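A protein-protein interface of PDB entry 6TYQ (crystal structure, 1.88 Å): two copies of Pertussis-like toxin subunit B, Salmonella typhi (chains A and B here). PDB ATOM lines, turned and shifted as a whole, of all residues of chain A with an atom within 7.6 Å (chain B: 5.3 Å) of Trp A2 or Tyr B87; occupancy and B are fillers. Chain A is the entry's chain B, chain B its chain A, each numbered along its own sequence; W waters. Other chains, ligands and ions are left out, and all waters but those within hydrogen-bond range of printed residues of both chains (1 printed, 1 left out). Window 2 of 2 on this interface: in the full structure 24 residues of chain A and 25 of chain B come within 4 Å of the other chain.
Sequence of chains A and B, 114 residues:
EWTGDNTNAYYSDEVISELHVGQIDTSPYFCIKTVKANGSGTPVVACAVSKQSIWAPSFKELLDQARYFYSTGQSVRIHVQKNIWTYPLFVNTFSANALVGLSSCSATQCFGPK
Water W1 bridges the side-chain carboxylate (OD1) of Asp A5 (2.8 Å) and the side-chain hydroxyl (OH) of Tyr B87 (2.8 Å).
Of the 14 printed residues of chain A, 7 touch a printed residue of chain B. Hydrophobic or aromatic side chains of chain A within 4 Å of the printed part of chain B: Trp A2 and Trp A55. Among the printed residues, no Asp or Glu carboxylate lies within 4 Å of a Lys or Arg side-chain nitrogen of the other chain.
Of the printed residues of chain A, Tyr B29 touches Trp A2 (2.8 Å) and Thr A3 (3.9 Å). Of the printed residues of chain A, Leu B89 touches Trp A2. The nearest residue of chain B that does not touch Trp A2 is Phe B94 (4.3 Å). The nearest residue of chain A that does not touch Tyr B87 is Asp A5 (4.7 Å).
Among the printed residues, merely in contact across the chains: Glu A1 with Ile B24 (3.3 Å), Trp A2 with Gln B23 (3.3 Å), Trp A2 with Ile B24 (3.8 Å), Trp A2 with Tyr B87 (3.8 Å), Trp A2 with Leu B89 (3.6 Å), Trp A2 with Phe B90 (3.8 Å), Trp A2 with Thr B93 (3.7 Å), Thr A3 with Tyr B29 (3.9 Å), Gly A112 with Thr B93 (3.8 Å), Gly A112 with Phe B94 (3.9 Å) and Pro A113 with Thr B93 (3.6 Å).
The backbone carbonyl oxygen (O) of Leu B89 sits at hydrogen-bond distance from the side-chain hydroxyl (OG1) of Thr B93, 3.0 Å away. The side-chain carboxylate (OD2) of Asp A5 lies within hydrogen-bond range of the backbone NH (N) of Trp A2 (2.9 Å). The backbone carbonyl oxygen (O) of Trp A2 sits at hydrogen-bond distance from the side-chain amide nitrogen (ND2) of Asn A8 (3.1 Å). The backbone carbonyl oxygen of Thr A3 sits at hydrogen-bond distance from the side-chain amide nitrogen of Asn A8 (3.1 Å). OG1 of Thr A3 lies within hydrogen-bond range of O of Val A100.
No position is printed for both chains.
NE2 of Gln B23 lies within hydrogen-bond range of O of Ile A54, 2.6 Å away. NE2 of Gln B23 lies within hydrogen-bond range of OE2 of Glu A1. The indole nitrogen (NE1) of Trp A2 sits at hydrogen-bond distance from the side-chain hydroxyl (OH) of Tyr B29 (2.8 Å). The side-chain amide oxygen (OE1) of Gln B23 lies close to the backbone carbonyl oxygen (O) of Trp A55 (3.3 Å). N of Asp B25 is in hydrogen-bond range of O of Glu A1 (2.9 Å). N of Gln B23 lies within hydrogen-bond range of OG1 of Thr A3 (2.9 Å).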
ATOM      1  N   GLU A   1     -12.416  -4.139   6.812  1.00  0.00           N
ATOM      2  CA  GLU A   1     -13.766  -4.284   6.288  1.00  0.00           C
ATOM      3  C   GLU A   1     -14.793  -3.834   7.328  1.00  0.00           C
ATOM      4  O   GLU A   1     -14.515  -3.825   8.532  1.00  0.00           O
ATOM      5  CB  GLU A   1     -14.026  -5.735   5.862  1.00  0.00           C
ATOM      6  CG  GLU A   1     -14.646  -6.630   6.935  1.00  0.00           C
ATOM      7  CD  GLU A   1     -13.720  -6.903   8.115  1.00  0.00           C
ATOM      8  OE1 GLU A   1     -12.529  -6.525   8.070  1.00  0.00           O
ATOM      9  OE2 GLU A   1     -14.191  -7.499   9.103  1.00  0.00           O
ATOM     10  N   TRP A   2     -15.980  -3.462   6.854  1.00  0.00           N
ATOM     11  CA  TRP A   2     -17.050  -3.006   7.731  1.00  0.00           C
ATOM     12  C   TRP A   2     -18.378  -3.185   7.012  1.00  0.00           C
ATOM     13  O   TRP A   2     -18.481  -2.919   5.811  1.00  0.00           O
ATOM     14  CB  TRP A   2     -16.870  -1.532   8.124  1.00  0.00           C
ATOM     15  CG  TRP A   2     -18.007  -0.944   8.937  1.00  0.00           C
ATOM     16  CD1 TRP A   2     -18.702  -1.543   9.961  1.00  0.00           C
ATOM     17  CD2 TRP A   2     -18.558   0.375   8.797  1.00  0.00           C
ATOM     18  NE1 TRP A   2     -19.657  -0.673  10.455  1.00  0.00           N
ATOM     19  CE2 TRP A   2     -19.587   0.506   9.757  1.00  0.00           C
ATOM     20  CE3 TRP A   2     -18.288   1.449   7.938  1.00  0.00           C
ATOM     21  CZ2 TRP A   2     -20.341   1.679   9.893  1.00  0.00           C
ATOM     22  CZ3 TRP A   2     -19.035   2.617   8.073  1.00  0.00           C
ATOM     23  CH2 TRP A   2     -20.054   2.718   9.036  1.00  0.00           C
ATOM     24  N   THR A   3     -19.383  -3.637   7.765  1.00  0.00           N
ATOM     25  CA  THR A   3     -20.768  -3.628   7.310  1.00  0.00           C
ATOM     26  C   THR A   3     -21.113  -2.380   6.499  1.00  0.00           C
ATOM     27  O   THR A   3     -21.755  -2.467   5.448  1.00  0.00           O
ATOM     28  CB  THR A   3     -21.694  -3.735   8.531  1.00  0.00           C
ATOM     29  OG1 THR A   3     -21.442  -4.971   9.203  1.00  0.00           O
ATOM     30  CG2 THR A   3     -23.149  -3.686   8.097  1.00  0.00           C
ATOM     31  N   GLY A   4     -20.699  -1.209   6.975  1.00  0.00           N
ATOM     32  CA  GLY A   4     -21.041   0.037   6.318  1.00  0.00           C
ATOM     33  C   GLY A   4     -20.176   0.450   5.143  1.00  0.00           C
ATOM     34  O   GLY A   4     -20.363   1.554   4.626  1.00  0.00           O
ATOM     35  N   ASP A   5     -19.232  -0.384   4.701  1.00  0.00           N
ATOM     36  CA  ASP A   5     -18.452  -0.059   3.509  1.00  0.00           C
ATOM     37  C   ASP A   5     -19.382   0.273   2.348  1.00  0.00           C
ATOM     38  O   ASP A   5     -20.412  -0.381   2.149  1.00  0.00           O
ATOM     39  CB  ASP A   5     -17.539  -1.228   3.114  1.00  0.00           C
ATOM     40  CG  ASP A   5     -16.379  -1.434   4.080  1.00  0.00           C
ATOM     41  OD1 ASP A   5     -16.032  -0.496   4.840  1.00  0.00           O
ATOM     42  OD2 ASP A   5     -15.805  -2.549   4.079  1.00  0.00           O
ATOM     43  N   ASN A   6     -19.010   1.292   1.566  1.00  0.00           N
ATOM     44  CA  ASN A   6     -19.856   1.680   0.437  1.00  0.00           C
ATOM     45  C   ASN A   6     -19.879   0.631  -0.672  1.00  0.00           C
ATOM     46  O   ASN A   6     -20.702   0.740  -1.590  1.00  0.00           O
ATOM     47  CB  ASN A   6     -19.419   3.050  -0.134  1.00  0.00           C
ATOM     48  CG  ASN A   6     -17.957   3.091  -0.536  1.00  0.00           C
ATOM     49  OD1 ASN A   6     -17.352   2.071  -0.854  1.00  0.00           O
ATOM     50  ND2 ASN A   6     -17.379   4.288  -0.524  1.00  0.00           N
ATOM     51  N   THR A   7     -19.021  -0.385  -0.607  1.00  0.00           N
ATOM     52  CA  THR A   7     -19.079  -1.492  -1.549  1.00  0.00           C
ATOM     53  C   THR A   7     -20.110  -2.558  -1.152  1.00  0.00           C
ATOM     54  O   THR A   7     -20.307  -3.527  -1.894  1.00  0.00           O
ATOM     55  CB  THR A   7     -17.695  -2.118  -1.690  1.00  0.00           C
ATOM     56  OG1 THR A   7     -17.168  -2.425  -0.391  1.00  0.00           O
ATOM     57  CG2 THR A   7     -16.763  -1.150  -2.385  1.00  0.00           C
ATOM     58  N   ASN A   8     -20.772  -2.400  -0.013  1.00  0.00           N
ATOM     59  CA  ASN A   8     -21.872  -3.272   0.373  1.00  0.00           C
ATOM     60  C   ASN A   8     -23.198  -2.618   0.011  1.00  0.00           C
ATOM     61  O   ASN A   8     -23.302  -1.392  -0.077  1.00  0.00           O
ATOM     62  CB  ASN A   8     -21.823  -3.578   1.869  1.00  0.00           C
ATOM     63  CG  ASN A   8     -20.577  -4.352   2.246  1.00  0.00           C
ATOM     64  OD1 ASN A   8     -20.113  -5.204   1.482  1.00  0.00           O
ATOM     65  ND2 ASN A   8     -20.029  -4.062   3.418  1.00  0.00           N
ATOM     66  N   ILE A  54     -15.230 -13.284   4.618  1.00  0.00           N
ATOM     67  CA  ILE A  54     -14.651 -12.461   5.669  1.00  0.00           C
ATOM     68  C   ILE A  54     -15.640 -12.196   6.793  1.00  0.00           C
ATOM     69  O   ILE A  54     -15.244 -11.756   7.876  1.00  0.00           O
ATOM     70  CB  ILE A  54     -14.130 -11.130   5.082  1.00  0.00           C
ATOM     71  CG1 ILE A  54     -13.146 -10.485   6.060  1.00  0.00           C
ATOM     72  CG2 ILE A  54     -15.280 -10.183   4.761  1.00  0.00           C
ATOM     73  CD1 ILE A  54     -12.383  -9.316   5.488  1.00  0.00           C
ATOM     74  N   TRP A  55     -16.919 -12.453   6.561  1.00  0.00           N
ATOM     75  CA  TRP A  55     -17.952 -12.237   7.564  1.00  0.00           C
ATOM     76  C   TRP A  55     -18.171 -13.445   8.465  1.00  0.00           C
ATOM     77  O   TRP A  55     -19.037 -13.393   9.345  1.00  0.00           O
ATOM     78  CB  TRP A  55     -19.262 -11.858   6.867  1.00  0.00           C
ATOM     79  CG  TRP A  55     -19.036 -10.818   5.814  1.00  0.00           C
ATOM     80  CD1 TRP A  55     -19.014 -11.011   4.463  1.00  0.00           C
ATOM     81  CD2 TRP A  55     -18.780  -9.430   6.025  1.00  0.00           C
ATOM     82  NE1 TRP A  55     -18.766  -9.830   3.817  1.00  0.00           N
ATOM     83  CE2 TRP A  55     -18.622  -8.837   4.751  1.00  0.00           C
ATOM     84  CE3 TRP A  55     -18.675  -8.625   7.168  1.00  0.00           C
ATOM     85  CZ2 TRP A  55     -18.363  -7.474   4.585  1.00  0.00           C
ATOM     86  CZ3 TRP A  55     -18.417  -7.273   7.005  1.00  0.00           C
ATOM     87  CH2 TRP A  55     -18.268  -6.708   5.726  1.00  0.00           C
ATOM     88  N   VAL A 100     -24.261  -9.217   5.923  1.00  0.00           N
ATOM     89  CA  VAL A 100     -23.192  -8.558   6.668  1.00  0.00           C
ATOM     90  C   VAL A 100     -23.695  -7.619   7.753  1.00  0.00           C
ATOM     91  O   VAL A 100     -22.875  -7.043   8.472  1.00  0.00           O
ATOM     92  CB  VAL A 100     -22.208  -7.812   5.739  1.00  0.00           C
ATOM     93  CG1 VAL A 100     -21.846  -8.688   4.555  1.00  0.00           C
ATOM     94  CG2 VAL A 100     -22.784  -6.482   5.265  1.00  0.00           C
ATOM     95  N   GLY A 112     -28.518   2.200  11.209  1.00  0.00           N
ATOM     96  CA  GLY A 112     -27.376   1.557  10.615  1.00  0.00           C
ATOM     97  C   GLY A 112     -26.823   2.379   9.477  1.00  0.00           C
ATOM     98  O   GLY A 112     -27.392   3.405   9.083  1.00  0.00           O
ATOM     99  N   PRO A 113     -25.707   1.926   8.911  1.00  0.00           N
ATOM    100  CA  PRO A 113     -25.037   2.699   7.859  1.00  0.00           C
ATOM    101  C   PRO A 113     -25.915   2.856   6.624  1.00  0.00           C
ATOM    102  O   PRO A 113     -26.809   2.050   6.349  1.00  0.00           O
ATOM    103  CB  PRO A 113     -23.785   1.867   7.527  1.00  0.00           C
ATOM    104  CG  PRO A 113     -23.759   0.719   8.473  1.00  0.00           C
ATOM    105  CD  PRO A 113     -25.065   0.627   9.188  1.00  0.00           C
ATOM    106  N   LYS A 114     -25.618   3.904   5.857  1.00  0.00           N
ATOM    107  CA  LYS A 114     -26.298   4.168   4.595  1.00  0.00           C
ATOM    108  C   LYS A 114     -25.340   4.957   3.717  1.00  0.00           C
ATOM    109  O   LYS A 114     -24.297   5.425   4.179  1.00  0.00           O
ATOM    110  CB  LYS A 114     -27.619   4.925   4.809  1.00  0.00           C
ATOM    111  CG  LYS A 114     -27.459   6.311   5.429  1.00  0.00           C
ATOM    112  CD  LYS A 114     -28.814   6.967   5.713  1.00  0.00           C
ATOM    113  CE  LYS A 114     -28.672   8.490   5.886  1.00  0.00           C
ATOM    114  NZ  LYS A 114     -28.774   8.937   7.310  1.00  0.00           N
ATOM    115  N   GLN B  23     -20.236  -6.232  11.488  1.00  0.00           N
ATOM    116  CA  GLN B  23     -18.848  -6.626  11.702  1.00  0.00           C
ATOM    117  C   GLN B  23     -17.934  -5.496  11.250  1.00  0.00           C
ATOM    118  O   GLN B  23     -18.232  -4.800  10.275  1.00  0.00           O
ATOM    119  CB  GLN B  23     -18.502  -7.914  10.939  1.00  0.00           C
ATOM    120  CG  GLN B  23     -17.050  -8.416  11.116  1.00  0.00           C
ATOM    121  CD  GLN B  23     -16.820  -9.742  10.405  1.00  0.00           C
ATOM    122  OE1 GLN B  23     -17.565 -10.706  10.612  1.00  0.00           O
ATOM    123  NE2 GLN B  23     -15.803  -9.797   9.564  1.00  0.00           N
ATOM    124  N   ILE B  24     -16.825  -5.318  11.960  1.00  0.00           N
ATOM    125  CA  ILE B  24     -15.798  -4.367  11.565  1.00  0.00           C
ATOM    126  C   ILE B  24     -14.442  -4.962  11.919  1.00  0.00           C
ATOM    127  O   ILE B  24     -14.253  -5.469  13.028  1.00  0.00           O
ATOM    128  CB  ILE B  24     -16.001  -2.986  12.228  1.00  0.00           C
ATOM    129  CG1 ILE B  24     -14.998  -1.973  11.666  1.00  0.00           C
ATOM    130  CG2 ILE B  24     -15.943  -3.087  13.773  1.00  0.00           C
ATOM    131  CD1 ILE B  24     -15.463  -0.541  11.784  1.00  0.00           C
ATOM    132  N   ASP B  25     -13.504  -4.922  10.968  1.00  0.00           N
ATOM    133  CA  ASP B  25     -12.123  -5.359  11.207  1.00  0.00           C
ATOM    134  C   ASP B  25     -12.069  -6.710  11.925  1.00  0.00           C
ATOM    135  O   ASP B  25     -11.361  -6.902  12.922  1.00  0.00           O
ATOM    136  CB  ASP B  25     -11.354  -4.273  11.965  1.00  0.00           C
ATOM    137  CG  ASP B  25     -11.189  -3.017  11.123  1.00  0.00           C
ATOM    138  OD1 ASP B  25     -11.122  -1.904  11.672  1.00  0.00           O
ATOM    139  OD2 ASP B  25     -11.162  -3.152   9.880  1.00  0.00           O
ATOM    140  N   TYR B  29     -19.824  -6.782  16.107  1.00  0.00           N
ATOM    141  CA  TYR B  29     -20.146  -5.685  17.011  1.00  0.00           C
ATOM    142  C   TYR B  29     -21.652  -5.505  17.024  1.00  0.00           C
ATOM    143  O   TYR B  29     -22.365  -5.994  16.149  1.00  0.00           O
ATOM    144  CB  TYR B  29     -19.454  -4.362  16.606  1.00  0.00           C
ATOM    145  CG  TYR B  29     -20.048  -3.705  15.361  1.00  0.00           C
ATOM    146  CD1 TYR B  29     -19.583  -4.028  14.090  1.00  0.00           C
ATOM    147  CD2 TYR B  29     -21.081  -2.771  15.461  1.00  0.00           C
ATOM    148  CE1 TYR B  29     -20.125  -3.434  12.953  1.00  0.00           C
ATOM    149  CE2 TYR B  29     -21.628  -2.174  14.333  1.00  0.00           C
ATOM    150  CZ  TYR B  29     -21.151  -2.514  13.083  1.00  0.00           C
ATOM    151  OH  TYR B  29     -21.707  -1.931  11.964  1.00  0.00           O
ATOM    152  N   TRP B  85     -14.495   4.614  20.287  1.00  0.00           N
ATOM    153  CA  TRP B  85     -14.368   4.207  18.889  1.00  0.00           C
ATOM    154  C   TRP B  85     -13.780   5.344  18.049  1.00  0.00           C
ATOM    155  O   TRP B  85     -13.997   6.527  18.327  1.00  0.00           O
ATOM    156  CB  TRP B  85     -15.729   3.756  18.344  1.00  0.00           C
ATOM    157  CG  TRP B  85     -16.428   2.829  19.332  1.00  0.00           C
ATOM    158  CD1 TRP B  85     -17.662   3.008  19.897  1.00  0.00           C
ATOM    159  CD2 TRP B  85     -15.896   1.626  19.902  1.00  0.00           C
ATOM    160  NE1 TRP B  85     -17.938   1.980  20.767  1.00  0.00           N
ATOM    161  CE2 TRP B  85     -16.866   1.122  20.797  1.00  0.00           C
ATOM    162  CE3 TRP B  85     -14.699   0.916  19.734  1.00  0.00           C
ATOM    163  CZ2 TRP B  85     -16.679  -0.059  21.518  1.00  0.00           C
ATOM    164  CZ3 TRP B  85     -14.520  -0.263  20.454  1.00  0.00           C
ATOM    165  CH2 TRP B  85     -15.505  -0.733  21.334  1.00  0.00           C
ATOM    166  N   THR B  86     -13.021   4.976  17.014  1.00  0.00           N
ATOM    167  CA  THR B  86     -12.243   5.957  16.256  1.00  0.00           C
ATOM    168  C   THR B  86     -12.489   5.974  14.747  1.00  0.00           C
ATOM    169  O   THR B  86     -12.222   7.007  14.119  1.00  0.00           O
ATOM    170  CB  THR B  86     -10.739   5.738  16.488  1.00  0.00           C
ATOM    171  OG1 THR B  86     -10.430   4.366  16.238  1.00  0.00           O
ATOM    172  CG2 THR B  86     -10.368   6.072  17.927  1.00  0.00           C
ATOM    173  N   TYR B  87     -12.953   4.885  14.134  1.00  0.00           N
ATOM    174  CA  TYR B  87     -13.181   4.937  12.689  1.00  0.00           C
ATOM    175  C   TYR B  87     -14.234   5.992  12.364  1.00  0.00           C
ATOM    176  O   TYR B  87     -15.406   5.829  12.738  1.00  0.00           O
ATOM    177  CB  TYR B  87     -13.601   3.562  12.149  1.00  0.00           C
ATOM    178  CG  TYR B  87     -13.653   3.475  10.635  1.00  0.00           C
ATOM    179  CD1 TYR B  87     -12.561   3.839   9.852  1.00  0.00           C
ATOM    180  CD2 TYR B  87     -14.793   3.049   9.990  1.00  0.00           C
ATOM    181  CE1 TYR B  87     -12.598   3.762   8.478  1.00  0.00           C
ATOM    182  CE2 TYR B  87     -14.841   2.981   8.607  1.00  0.00           C
ATOM    183  CZ  TYR B  87     -13.745   3.345   7.863  1.00  0.00           C
ATOM    184  OH  TYR B  87     -13.800   3.277   6.496  1.00  0.00           O
ATOM    185  N   PRO B  88     -13.871   7.080  11.658  1.00  0.00           N
ATOM    186  CA  PRO B  88     -14.810   8.207  11.531  1.00  0.00           C
ATOM    187  C   PRO B  88     -16.154   7.830  10.951  1.00  0.00           C
ATOM    188  O   PRO B  88     -17.180   8.291  11.455  1.00  0.00           O
ATOM    189  CB  PRO B  88     -14.049   9.189  10.624  1.00  0.00           C
ATOM    190  CG  PRO B  88     -12.619   8.869  10.865  1.00  0.00           C
ATOM    191  CD  PRO B  88     -12.600   7.379  10.987  1.00  0.00           C
ATOM    192  N   LEU B  89     -16.191   7.009   9.900  1.00  0.00           N
ATOM    193  CA  LEU B  89     -17.482   6.670   9.310  1.00  0.00           C
ATOM    194  C   LEU B  89     -18.340   5.884  10.293  1.00  0.00           C
ATOM    195  O   LEU B  89     -19.566   6.057  10.332  1.00  0.00           O
ATOM    196  CB  LEU B  89     -17.281   5.891   8.011  1.00  0.00           C
ATOM    197  CG  LEU B  89     -16.708   6.759   6.876  1.00  0.00           C
ATOM    198  CD1 LEU B  89     -16.335   5.916   5.668  1.00  0.00           C
ATOM    199  CD2 LEU B  89     -17.693   7.854   6.478  1.00  0.00           C
ATOM    200  N   PHE B  90     -17.712   5.022  11.099  1.00  0.00           N
ATOM    201  CA  PHE B  90     -18.427   4.293  12.147  1.00  0.00           C
ATOM    202  C   PHE B  90     -18.935   5.253  13.217  1.00  0.00           C
ATOM    203  O   PHE B  90     -20.113   5.219  13.595  1.00  0.00           O
ATOM    204  CB  PHE B  90     -17.499   3.233  12.757  1.00  0.00           C
ATOM    205  CG  PHE B  90     -18.135   2.389  13.848  1.00  0.00           C
ATOM    206  CD1 PHE B  90     -18.297   2.881  15.130  1.00  0.00           C
ATOM    207  CD2 PHE B  90     -18.534   1.089  13.585  1.00  0.00           C
ATOM    208  CE1 PHE B  90     -18.863   2.102  16.136  1.00  0.00           C
ATOM    209  CE2 PHE B  90     -19.098   0.291  14.586  1.00  0.00           C
ATOM    210  CZ  PHE B  90     -19.272   0.801  15.860  1.00  0.00           C
ATOM    211  N   VAL B  91     -18.051   6.116  13.720  1.00  0.00           N
ATOM    212  CA  VAL B  91     -18.450   7.076  14.745  1.00  0.00           C
ATOM    213  C   VAL B  91     -19.559   7.980  14.225  1.00  0.00           C
ATOM    214  O   VAL B  91     -20.501   8.294  14.951  1.00  0.00           O
ATOM    215  CB  VAL B  91     -17.234   7.886  15.236  1.00  0.00           C
ATOM    216  CG1 VAL B  91     -17.687   9.013  16.167  1.00  0.00           C
ATOM    217  CG2 VAL B  91     -16.263   6.975  15.973  1.00  0.00           C
ATOM    218  N   ASN B  92     -19.494   8.388  12.949  1.00  0.00           N
ATOM    219  CA  ASN B  92     -20.544   9.261  12.424  1.00  0.00           C
ATOM    220  C   ASN B  92     -21.875   8.528  12.268  1.00  0.00           C
ATOM    221  O   ASN B  92     -22.944   9.128  12.443  1.00  0.00           O
ATOM    222  CB  ASN B  92     -20.117   9.865  11.086  1.00  0.00           C
ATOM    223  CG  ASN B  92     -21.112  10.883  10.570  1.00  0.00           C
ATOM    224  OD1 ASN B  92     -21.298  11.942  11.176  1.00  0.00           O
ATOM    225  ND2 ASN B  92     -21.767  10.567   9.453  1.00  0.00           N
ATOM    226  N   THR B  93     -21.843   7.242  11.934  1.00  0.00           N
ATOM    227  CA  THR B  93     -23.086   6.477  11.853  1.00  0.00           C
ATOM    228  C   THR B  93     -23.677   6.223  13.238  1.00  0.00           C
ATOM    229  O   THR B  93     -24.900   6.292  13.429  1.00  0.00           O
ATOM    230  CB  THR B  93     -22.803   5.163  11.124  1.00  0.00           C
ATOM    231  OG1 THR B  93     -22.407   5.456   9.777  1.00  0.00           O
ATOM    232  CG2 THR B  93     -24.014   4.241  11.125  1.00  0.00           C
ATOM    233  N   PHE B  94     -22.822   5.934  14.221  1.00  0.00           N
ATOM    234  CA  PHE B  94     -23.267   5.483  15.531  1.00  0.00           C
ATOM    235  C   PHE B  94     -22.763   6.494  16.548  1.00  0.00           C
ATOM    236  O   PHE B  94     -23.363   7.562  16.702  1.00  0.00           O
ATOM    237  CB  PHE B  94     -22.779   4.052  15.799  1.00  0.00           C
ATOM    238  CG  PHE B  94     -23.370   3.021  14.860  1.00  0.00           C
ATOM    239  CD1 PHE B  94     -24.725   2.769  14.849  1.00  0.00           C
ATOM    240  CD2 PHE B  94     -22.556   2.310  13.997  1.00  0.00           C
ATOM    241  CE1 PHE B  94     -25.271   1.808  13.995  1.00  0.00           C
ATOM    242  CE2 PHE B  94     -23.086   1.369  13.144  1.00  0.00           C
ATOM    243  CZ  PHE B  94     -24.447   1.114  13.142  1.00  0.00           C
HETATM  244  O   HOH W   1     -16.027   2.251   5.150  1.00  0.00           O
